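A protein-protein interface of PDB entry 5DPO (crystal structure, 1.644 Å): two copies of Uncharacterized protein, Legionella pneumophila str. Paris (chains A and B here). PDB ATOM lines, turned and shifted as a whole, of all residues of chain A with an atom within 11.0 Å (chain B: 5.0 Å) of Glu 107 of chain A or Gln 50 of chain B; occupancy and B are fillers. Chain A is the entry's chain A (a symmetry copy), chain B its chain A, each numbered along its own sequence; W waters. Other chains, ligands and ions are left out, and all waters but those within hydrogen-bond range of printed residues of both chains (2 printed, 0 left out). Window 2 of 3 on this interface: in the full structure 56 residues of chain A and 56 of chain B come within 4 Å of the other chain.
Of the 17 printed residues of chain A, 7 touch a printed residue of chain B.
Printed residues of chain A that touch a printed residue of chain B: Ile 99, Lys 100, Ala 103, Arg 104, Ile 106, Glu 107 and Thr 111.
Hydrophobic or aromatic side chains of chain B that line the printed part of chain A: Leu 46, Leu 49 and Leu 52.
Among the printed residues, 8 pairs touch across the chains.
Among the printed residues, no Asp or Glu carboxylate lies within 4 Å of a Lys or Arg side-chain nitrogen of the other chain.
Leu 52 of chain B touches Ile 99 of chain A.
Leu 52 of chain B touches Lys 100 of chain A.
Ser 53 of chain B touches Lys 100 of chain A (O to CE, 3.2 Å).
CD1 of Leu 49 of chain B touches CB of Ala 103 of chain A (3.6 Å).
Arg 104 of chain A touches Ser 53 of chain B.
CD2 of Leu 49 of chain B touches CG2 of Ile 106 of chain A (3.8 Å).
Leu 46 of chain B touches Thr 111 of chain A.
Water W2 lies within hydrogen-bond range of the side-chain hydroxyl (OG) of Ser 53 of chain B, the side-chain carboxylate (OE1) of Glu 107 of chain A and the guanidinium group (NH1) of Arg 104 of chain A.
Water W1 bridges the backbone carbonyl oxygen of Ser 53 of chain B (3.0 Å) and the backbone carbonyl oxygen of Lys 100 of chain A (3.5 Å).
Leu 98 of chain A touches none of the printed residues of chain B.
Of the printed residues of chain B, Ile 106 of chain A touches Leu 49 (3.8 Å).
Glu 107 of chain A touches just one residue of chain B: Gln 50 (2.9 Å).
No residue of chain A comes within 4 Å of Lys 47 of chain B.
No residue of chain A comes within 4 Å of Ser 48 of chain B.
Leu 49 of chain B touches just these residues of chain A: Ala 103 (3.6 Å) and Ile 106 (3.8 Å).
Of chain A, only Glu 107 (2.9 Å) comes within 4 Å of Gln 50 of chain B.
Of the printed residues of chain A, Ser 53 of chain B touches Lys 100 and Arg 104.
The nearest residue of chain A that does not touch Gln 50 of chain B is Thr 111 of chain A (5.1 Å).
The nearest printed residue of chain A that does not touch Leu 52 of chain B is Ala 103 of chain A (4.1 Å).
The side-chain amide nitrogen of Gln 50 of chain B sits at hydrogen-bond distance from the side-chain carboxylate of Glu 107 of chain A.
No position is printed for both chains.
Of the 8 pairs that touch across the chains among the printed residues, none has its exchanged pair printed and touching as well.
The guanidinium group (NH1) of Arg 104 of chain A lies within salt-bridge range of the side-chain carboxylate (OE1) of Glu 107 of chain A (3.1 Å).
O of Thr 111 of chain A lies close to OE1 of Gln 113 of chain A, at 3.1 Å.
The backbone carbonyl oxygen (O) of Gln 50 of chain B is in hydrogen-bond range of the side-chain hydroxyl (OG) of Ser 53 of chain B (2.7 Å).
O of Glu 107 of chain A is in hydrogen-bond range of OG1 of Thr 111 of chain A.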
ATOM      1  N   LEU A  98      -7.103  -2.272  11.716  1.00  0.00           N
ATOM      2  CA  LEU A  98      -5.745  -2.336  11.183  1.00  0.00           C
ATOM      3  C   LEU A  98      -5.597  -3.484  10.190  1.00  0.00           C
ATOM      4  O   LEU A  98      -4.980  -3.334   9.132  1.00  0.00           O
ATOM      5  CB  LEU A  98      -4.724  -2.492  12.317  1.00  0.00           C
ATOM      6  CG  LEU A  98      -3.282  -2.766  11.883  1.00  0.00           C
ATOM      7  CD1 LEU A  98      -2.700  -1.546  11.191  1.00  0.00           C
ATOM      8  CD2 LEU A  98      -2.426  -3.161  13.086  1.00  0.00           C
ATOM      9  N   ILE A  99      -6.163  -4.635  10.533  1.00  0.00           N
ATOM     10  CA  ILE A  99      -6.125  -5.785   9.634  1.00  0.00           C
ATOM     11  C   ILE A  99      -6.828  -5.485   8.306  1.00  0.00           C
ATOM     12  O   ILE A  99      -6.292  -5.781   7.249  1.00  0.00           O
ATOM     13  CB  ILE A  99      -6.755  -7.023  10.290  1.00  0.00           C
ATOM     14  CG1 ILE A  99      -5.869  -7.503  11.450  1.00  0.00           C
ATOM     15  CG2 ILE A  99      -6.918  -8.137   9.283  1.00  0.00           C
ATOM     16  CD1 ILE A  99      -6.550  -8.520  12.346  1.00  0.00           C
ATOM     17  N   LYS A 100      -8.016  -4.888   8.357  1.00  0.00           N
ATOM     18  CA  LYS A 100      -8.725  -4.529   7.126  1.00  0.00           C
ATOM     19  C   LYS A 100      -7.945  -3.511   6.299  1.00  0.00           C
ATOM     20  O   LYS A 100      -7.838  -3.640   5.076  1.00  0.00           O
ATOM     21  CB  LYS A 100     -10.113  -3.969   7.433  1.00  0.00           C
ATOM     22  CG  LYS A 100     -11.062  -4.977   8.061  1.00  0.00           C
ATOM     23  CD  LYS A 100     -12.359  -4.314   8.516  1.00  0.00           C
ATOM     24  CE  LYS A 100     -13.107  -3.717   7.332  1.00  0.00           C
ATOM     25  NZ  LYS A 100     -14.422  -3.174   7.755  1.00  0.00           N
ATOM     26  N   GLU A 101      -7.404  -2.499   6.972  1.00  0.00           N
ATOM     27  CA  GLU A 101      -6.637  -1.454   6.290  1.00  0.00           C
ATOM     28  C   GLU A 101      -5.393  -2.023   5.621  1.00  0.00           C
ATOM     29  O   GLU A 101      -5.045  -1.646   4.503  1.00  0.00           O
ATOM     30  CB  GLU A 101      -6.243  -0.348   7.276  1.00  0.00           C
ATOM     31  CG  GLU A 101      -7.408   0.537   7.693  1.00  0.00           C
ATOM     32  CD  GLU A 101      -7.074   1.412   8.889  1.00  0.00           C
ATOM     33  OE1 GLU A 101      -5.934   1.316   9.401  1.00  0.00           O
ATOM     34  OE2 GLU A 101      -7.953   2.188   9.322  1.00  0.00           O
ATOM     35  N   THR A 102      -4.732  -2.940   6.317  1.00  0.00           N
ATOM     36  CA  THR A 102      -3.517  -3.555   5.817  1.00  0.00           C
ATOM     37  C   THR A 102      -3.823  -4.485   4.652  1.00  0.00           C
ATOM     38  O   THR A 102      -3.101  -4.498   3.653  1.00  0.00           O
ATOM     39  CB  THR A 102      -2.804  -4.320   6.938  1.00  0.00           C
ATOM     40  OG1 THR A 102      -2.495  -3.404   7.993  1.00  0.00           O
ATOM     41  CG2 THR A 102      -1.519  -4.954   6.428  1.00  0.00           C
ATOM     42  N   ALA A 103      -4.903  -5.251   4.774  1.00  0.00           N
ATOM     43  CA  ALA A 103      -5.350  -6.118   3.686  1.00  0.00           C
ATOM     44  C   ALA A 103      -5.576  -5.311   2.408  1.00  0.00           C
ATOM     45  O   ALA A 103      -5.169  -5.723   1.325  1.00  0.00           O
ATOM     46  CB  ALA A 103      -6.622  -6.859   4.079  1.00  0.00           C
ATOM     47  N   ARG A 104      -6.223  -4.158   2.546  1.00  0.00           N
ATOM     48  CA  ARG A 104      -6.506  -3.297   1.403  1.00  0.00           C
ATOM     49  C   ARG A 104      -5.224  -2.723   0.804  1.00  0.00           C
ATOM     50  O   ARG A 104      -5.063  -2.706  -0.421  1.00  0.00           O
ATOM     51  CB  ARG A 104      -7.453  -2.168   1.813  1.00  0.00           C
ATOM     52  CG  ARG A 104      -7.692  -1.110   0.736  1.00  0.00           C
ATOM     53  CD  ARG A 104      -8.358  -1.674  -0.507  1.00  0.00           C
ATOM     54  NE  ARG A 104      -8.712  -0.595  -1.422  1.00  0.00           N
ATOM     55  CZ  ARG A 104      -9.179  -0.774  -2.653  1.00  0.00           C
ATOM     56  NH1 ARG A 104      -9.351  -1.996  -3.134  1.00  0.00           N
ATOM     57  NH2 ARG A 104      -9.466   0.279  -3.409  1.00  0.00           N
ATOM     58  N   GLU A 105      -4.316  -2.265   1.663  1.00  0.00           N
ATOM     59  CA  GLU A 105      -3.027  -1.744   1.202  1.00  0.00           C
ATOM     60  C   GLU A 105      -2.258  -2.791   0.399  1.00  0.00           C
ATOM     61  O   GLU A 105      -1.761  -2.515  -0.700  1.00  0.00           O
ATOM     62  CB  GLU A 105      -2.184  -1.265   2.386  1.00  0.00           C
ATOM     63  CG  GLU A 105      -2.679   0.037   2.998  1.00  0.00           C
ATOM     64  CD  GLU A 105      -1.907   0.446   4.242  1.00  0.00           C
ATOM     65  OE1 GLU A 105      -1.177  -0.394   4.808  1.00  0.00           O
ATOM     66  OE2 GLU A 105      -2.026   1.620   4.645  1.00  0.00           O
ATOM     67  N   ILE A 106      -2.171  -3.996   0.949  1.00  0.00           N
ATOM     68  CA  ILE A 106      -1.463  -5.080   0.286  1.00  0.00           C
ATOM     69  C   ILE A 106      -2.122  -5.414  -1.048  1.00  0.00           C
ATOM     70  O   ILE A 106      -1.431  -5.605  -2.046  1.00  0.00           O
ATOM     71  CB  ILE A 106      -1.394  -6.335   1.177  1.00  0.00           C
ATOM     72  CG1 ILE A 106      -0.481  -6.061   2.375  1.00  0.00           C
ATOM     73  CG2 ILE A 106      -0.873  -7.527   0.385  1.00  0.00           C
ATOM     74  CD1 ILE A 106      -0.581  -7.086   3.498  1.00  0.00           C
ATOM     75  N   GLU A 107      -3.451  -5.462  -1.068  1.00  0.00           N
ATOM     76  CA  GLU A 107      -4.176  -5.721  -2.309  1.00  0.00           C
ATOM     77  C   GLU A 107      -3.770  -4.730  -3.398  1.00  0.00           C
ATOM     78  O   GLU A 107      -3.483  -5.125  -4.526  1.00  0.00           O
ATOM     79  CB  GLU A 107      -5.691  -5.648  -2.100  1.00  0.00           C
ATOM     80  CG  GLU A 107      -6.480  -5.851  -3.398  1.00  0.00           C
ATOM     81  CD  GLU A 107      -7.886  -5.284  -3.349  1.00  0.00           C
ATOM     82  OE1 GLU A 107      -8.302  -4.786  -2.279  1.00  0.00           O
ATOM     83  OE2 GLU A 107      -8.576  -5.330  -4.392  1.00  0.00           O
ATOM     84  N   LEU A 108      -3.749  -3.444  -3.059  1.00  0.00           N
ATOM     85  CA  LEU A 108      -3.445  -2.419  -4.061  1.00  0.00           C
ATOM     86  C   LEU A 108      -2.014  -2.530  -4.586  1.00  0.00           C
ATOM     87  O   LEU A 108      -1.764  -2.280  -5.764  1.00  0.00           O
ATOM     88  CB  LEU A 108      -3.695  -1.021  -3.489  1.00  0.00           C
ATOM     89  CG  LEU A 108      -5.182  -0.719  -3.269  1.00  0.00           C
ATOM     90  CD1 LEU A 108      -5.355   0.573  -2.496  1.00  0.00           C
ATOM     91  CD2 LEU A 108      -5.947  -0.672  -4.601  1.00  0.00           C
ATOM     92  N   VAL A 109      -1.077  -2.918  -3.724  1.00  0.00           N
ATOM     93  CA  VAL A 109       0.310  -3.085  -4.148  1.00  0.00           C
ATOM     94  C   VAL A 109       0.485  -4.356  -4.973  1.00  0.00           C
ATOM     95  O   VAL A 109       1.086  -4.328  -6.053  1.00  0.00           O
ATOM     96  CB  VAL A 109       1.262  -3.110  -2.931  1.00  0.00           C
ATOM     97  CG1 VAL A 109       2.687  -3.445  -3.347  1.00  0.00           C
ATOM     98  CG2 VAL A 109       1.220  -1.769  -2.227  1.00  0.00           C
ATOM     99  N   PHE A 110      -0.061  -5.460  -4.468  1.00  0.00           N
ATOM    100  CA  PHE A 110       0.070  -6.755  -5.123  1.00  0.00           C
ATOM    101  C   PHE A 110      -0.562  -6.766  -6.511  1.00  0.00           C
ATOM    102  O   PHE A 110      -0.057  -7.426  -7.420  1.00  0.00           O
ATOM    103  CB  PHE A 110      -0.555  -7.852  -4.245  1.00  0.00           C
ATOM    104  CG  PHE A 110      -0.433  -9.233  -4.823  1.00  0.00           C
ATOM    105  CD1 PHE A 110       0.780  -9.897  -4.807  1.00  0.00           C
ATOM    106  CD2 PHE A 110      -1.536  -9.871  -5.368  1.00  0.00           C
ATOM    107  CE1 PHE A 110       0.896 -11.175  -5.339  1.00  0.00           C
ATOM    108  CE2 PHE A 110      -1.424 -11.149  -5.902  1.00  0.00           C
ATOM    109  CZ  PHE A 110      -0.213 -11.794  -5.886  1.00  0.00           C
ATOM    110  N   THR A 111      -1.660  -6.033  -6.674  1.00  0.00           N
ATOM    111  CA  THR A 111      -2.337  -5.957  -7.969  1.00  0.00           C
ATOM    112  C   THR A 111      -1.863  -4.764  -8.802  1.00  0.00           C
ATOM    113  O   THR A 111      -2.442  -4.461  -9.849  1.00  0.00           O
ATOM    114  CB  THR A 111      -3.871  -5.883  -7.808  1.00  0.00           C
ATOM    115  OG1 THR A 111      -4.229  -4.715  -7.054  1.00  0.00           O
ATOM    116  CG2 THR A 111      -4.391  -7.126  -7.090  1.00  0.00           C
ATOM    117  N   HIS A 112      -0.815  -4.090  -8.333  1.00  0.00           N
ATOM    118  CA  HIS A 112      -0.171  -2.997  -9.070  1.00  0.00           C
ATOM    119  C   HIS A 112      -1.112  -1.838  -9.376  1.00  0.00           C
ATOM    120  O   HIS A 112      -1.020  -1.211 -10.436  1.00  0.00           O
ATOM    121  CB  HIS A 112       0.449  -3.524 -10.368  1.00  0.00           C
ATOM    122  CG  HIS A 112       1.626  -4.418 -10.146  1.00  0.00           C
ATOM    123  ND1 HIS A 112       2.798  -4.298 -10.861  1.00  0.00           N
ATOM    124  CD2 HIS A 112       1.819  -5.440  -9.279  1.00  0.00           C
ATOM    125  CE1 HIS A 112       3.658  -5.209 -10.448  1.00  0.00           C
ATOM    126  NE2 HIS A 112       3.092  -5.914  -9.485  1.00  0.00           N
ATOM    127  N   GLN A 113      -2.006  -1.544  -8.434  1.00  0.00           N
ATOM    128  CA  GLN A 113      -2.890  -0.390  -8.552  1.00  0.00           C
ATOM    129  C   GLN A 113      -2.203   0.841  -7.975  1.00  0.00           C
ATOM    130  O   GLN A 113      -2.514   1.967  -8.343  1.00  0.00           O
ATOM    131  CB  GLN A 113      -4.218  -0.636  -7.835  1.00  0.00           C
ATOM    132  CG  GLN A 113      -5.005  -1.845  -8.338  1.00  0.00           C
ATOM    133  CD  GLN A 113      -5.316  -1.771  -9.816  1.00  0.00           C
ATOM    134  OE1 GLN A 113      -4.691  -2.456 -10.628  1.00  0.00           O
ATOM    135  NE2 GLN A 113      -6.279  -0.939 -10.174  1.00  0.00           N
ATOM    136  N   LYS A 114      -1.259   0.602  -7.072  1.00  0.00           N
ATOM    137  CA  LYS A 114      -0.512   1.671  -6.428  1.00  0.00           C
ATOM    138  C   LYS A 114       0.981   1.446  -6.613  1.00  0.00           C
ATOM    139  O   LYS A 114       1.503   0.406  -6.204  1.00  0.00           O
ATOM    140  CB  LYS A 114      -0.861   1.736  -4.945  1.00  0.00           C
ATOM    141  CG  LYS A 114       0.033   2.651  -4.118  1.00  0.00           C
ATOM    142  CD  LYS A 114      -0.485   2.761  -2.691  1.00  0.00           C
ATOM    143  CE  LYS A 114       0.570   3.312  -1.750  1.00  0.00           C
ATOM    144  NZ  LYS A 114       1.231   4.532  -2.290  1.00  0.00           N
ATOM    145  N   LEU B  46      -5.922 -14.117  -3.111  1.00  0.00           N
ATOM    146  CA  LEU B  46      -6.188 -12.695  -3.283  1.00  0.00           C
ATOM    147  C   LEU B  46      -7.647 -12.386  -2.969  1.00  0.00           C
ATOM    148  O   LEU B  46      -7.947 -11.377  -2.336  1.00  0.00           O
ATOM    149  CB  LEU B  46      -5.837 -12.243  -4.704  1.00  0.00           C
ATOM    150  CG  LEU B  46      -6.215 -10.801  -5.050  1.00  0.00           C
ATOM    151  CD1 LEU B  46      -5.514  -9.807  -4.123  1.00  0.00           C
ATOM    152  CD2 LEU B  46      -5.883 -10.509  -6.501  1.00  0.00           C
ATOM    153  N   LYS B  47      -8.552 -13.260  -3.400  1.00  0.00           N
ATOM    154  CA  LYS B  47      -9.968 -13.048  -3.140  1.00  0.00           C
ATOM    155  C   LYS B  47     -10.261 -13.082  -1.646  1.00  0.00           C
ATOM    156  O   LYS B  47     -11.046 -12.277  -1.150  1.00  0.00           O
ATOM    157  CB  LYS B  47     -10.825 -14.086  -3.862  1.00  0.00           C
ATOM    158  CG  LYS B  47     -12.320 -13.896  -3.636  1.00  0.00           C
ATOM    159  CD  LYS B  47     -12.777 -12.516  -4.089  1.00  0.00           C
ATOM    160  CE  LYS B  47     -14.261 -12.312  -3.837  1.00  0.00           C
ATOM    161  NZ  LYS B  47     -14.693 -10.926  -4.176  1.00  0.00           N
ATOM    162  N   SER B  48      -9.626 -13.998  -0.922  1.00  0.00           N
ATOM    163  CA  SER B  48      -9.849 -14.063   0.520  1.00  0.00           C
ATOM    164  C   SER B  48      -9.346 -12.794   1.202  1.00  0.00           C
ATOM    165  O   SER B  48      -9.931 -12.340   2.188  1.00  0.00           O
ATOM    166  CB  SER B  48      -9.178 -15.294   1.127  1.00  0.00           C
ATOM    167  OG  SER B  48      -7.778 -15.120   1.210  1.00  0.00           O
ATOM    168  N   LEU B  49      -8.262 -12.226   0.674  1.00  0.00           N
ATOM    169  CA  LEU B  49      -7.716 -10.986   1.208  1.00  0.00           C
ATOM    170  C   LEU B  49      -8.631  -9.803   0.890  1.00  0.00           C
ATOM    171  O   LEU B  49      -8.809  -8.912   1.720  1.00  0.00           O
ATOM    172  CB  LEU B  49      -6.304 -10.733   0.659  1.00  0.00           C
ATOM    173  CG  LEU B  49      -5.528  -9.575   1.297  1.00  0.00           C
ATOM    174  CD1 LEU B  49      -5.200  -9.852   2.771  1.00  0.00           C
ATOM    175  CD2 LEU B  49      -4.259  -9.269   0.508  1.00  0.00           C
ATOM    176  N   GLN B  50      -9.205  -9.793  -0.310  1.00  0.00           N
ATOM    177  CA  GLN B  50     -10.179  -8.760  -0.664  1.00  0.00           C
ATOM    178  C   GLN B  50     -11.421  -8.862   0.214  1.00  0.00           C
ATOM    179  O   GLN B  50     -11.946  -7.846   0.672  1.00  0.00           O
ATOM    180  CB  GLN B  50     -10.559  -8.842  -2.152  1.00  0.00           C
ATOM    181  CG  GLN B  50      -9.375  -8.535  -3.062  1.00  0.00           C
ATOM    182  CD  GLN B  50      -9.622  -8.879  -4.521  1.00  0.00           C
ATOM    183  OE1 GLN B  50     -10.188  -9.927  -4.848  1.00  0.00           O
ATOM    184  NE2 GLN B  50      -9.174  -8.000  -5.413  1.00  0.00           N
ATOM    185  N   GLU B  51     -11.887 -10.081   0.460  1.00  0.00           N
ATOM    186  CA  GLU B  51     -12.992 -10.281   1.400  1.00  0.00           C
ATOM    187  C   GLU B  51     -12.657  -9.732   2.777  1.00  0.00           C
ATOM    188  O   GLU B  51     -13.481  -9.071   3.412  1.00  0.00           O
ATOM    189  CB  GLU B  51     -13.341 -11.759   1.530  1.00  0.00           C
ATOM    190  CG  GLU B  51     -14.112 -12.320   0.371  1.00  0.00           C
ATOM    191  CD  GLU B  51     -14.295 -13.816   0.475  1.00  0.00           C
ATOM    192  OE1 GLU B  51     -13.717 -14.439   1.401  1.00  0.00           O
ATOM    193  OE2 GLU B  51     -15.018 -14.366  -0.377  1.00  0.00           O
ATOM    194  N   LEU B  52     -11.449 -10.029   3.246  1.00  0.00           N
ATOM    195  CA  LEU B  52     -11.026  -9.599   4.575  1.00  0.00           C
ATOM    196  C   LEU B  52     -11.105  -8.074   4.707  1.00  0.00           C
ATOM    197  O   LEU B  52     -11.562  -7.555   5.728  1.00  0.00           O
ATOM    198  CB  LEU B  52      -9.607 -10.089   4.874  1.00  0.00           C
ATOM    199  CG  LEU B  52      -9.001  -9.715   6.228  1.00  0.00           C
ATOM    200  CD1 LEU B  52      -9.835 -10.277   7.380  1.00  0.00           C
ATOM    201  CD2 LEU B  52      -7.567 -10.219   6.305  1.00  0.00           C
ATOM    202  N   SER B  53     -10.696  -7.357   3.661  1.00  0.00           N
ATOM    203  CA  SER B  53     -10.705  -5.894   3.703  1.00  0.00           C
ATOM    204  C   SER B  53     -12.117  -5.321   3.848  1.00  0.00           C
ATOM    205  O   SER B  53     -12.278  -4.173   4.248  1.00  0.00           O
ATOM    206  CB  SER B  53     -10.032  -5.317   2.446  1.00  0.00           C
ATOM    207  OG  SER B  53     -10.871  -5.424   1.299  1.00  0.00           O
ATOM    208  N   GLU B  54     -13.131  -6.125   3.528  1.00  0.00           N
ATOM    209  CA  GLU B  54     -14.523  -5.687   3.580  1.00  0.00           C
ATOM    210  C   GLU B  54     -15.305  -6.320   4.734  1.00  0.00           C
ATOM    211  O   GLU B  54     -16.509  -6.103   4.853  1.00  0.00           O
ATOM    212  CB  GLU B  54     -15.237  -6.011   2.260  1.00  0.00           C
ATOM    213  CG  GLU B  54     -14.539  -5.493   1.013  1.00  0.00           C
ATOM    214  CD  GLU B  54     -15.388  -5.659  -0.235  1.00  0.00           C
ATOM    215  OE1 GLU B  54     -16.232  -6.579  -0.266  1.00  0.00           O
ATOM    216  OE2 GLU B  54     -15.213  -4.866  -1.184  1.00  0.00           O
HETATM  217  O   HOH W   1     -10.513  -1.826   3.807  1.00  0.00           O
HETATM  218  O   HOH W   2     -10.836  -4.435  -1.157  1.00  0.00           O
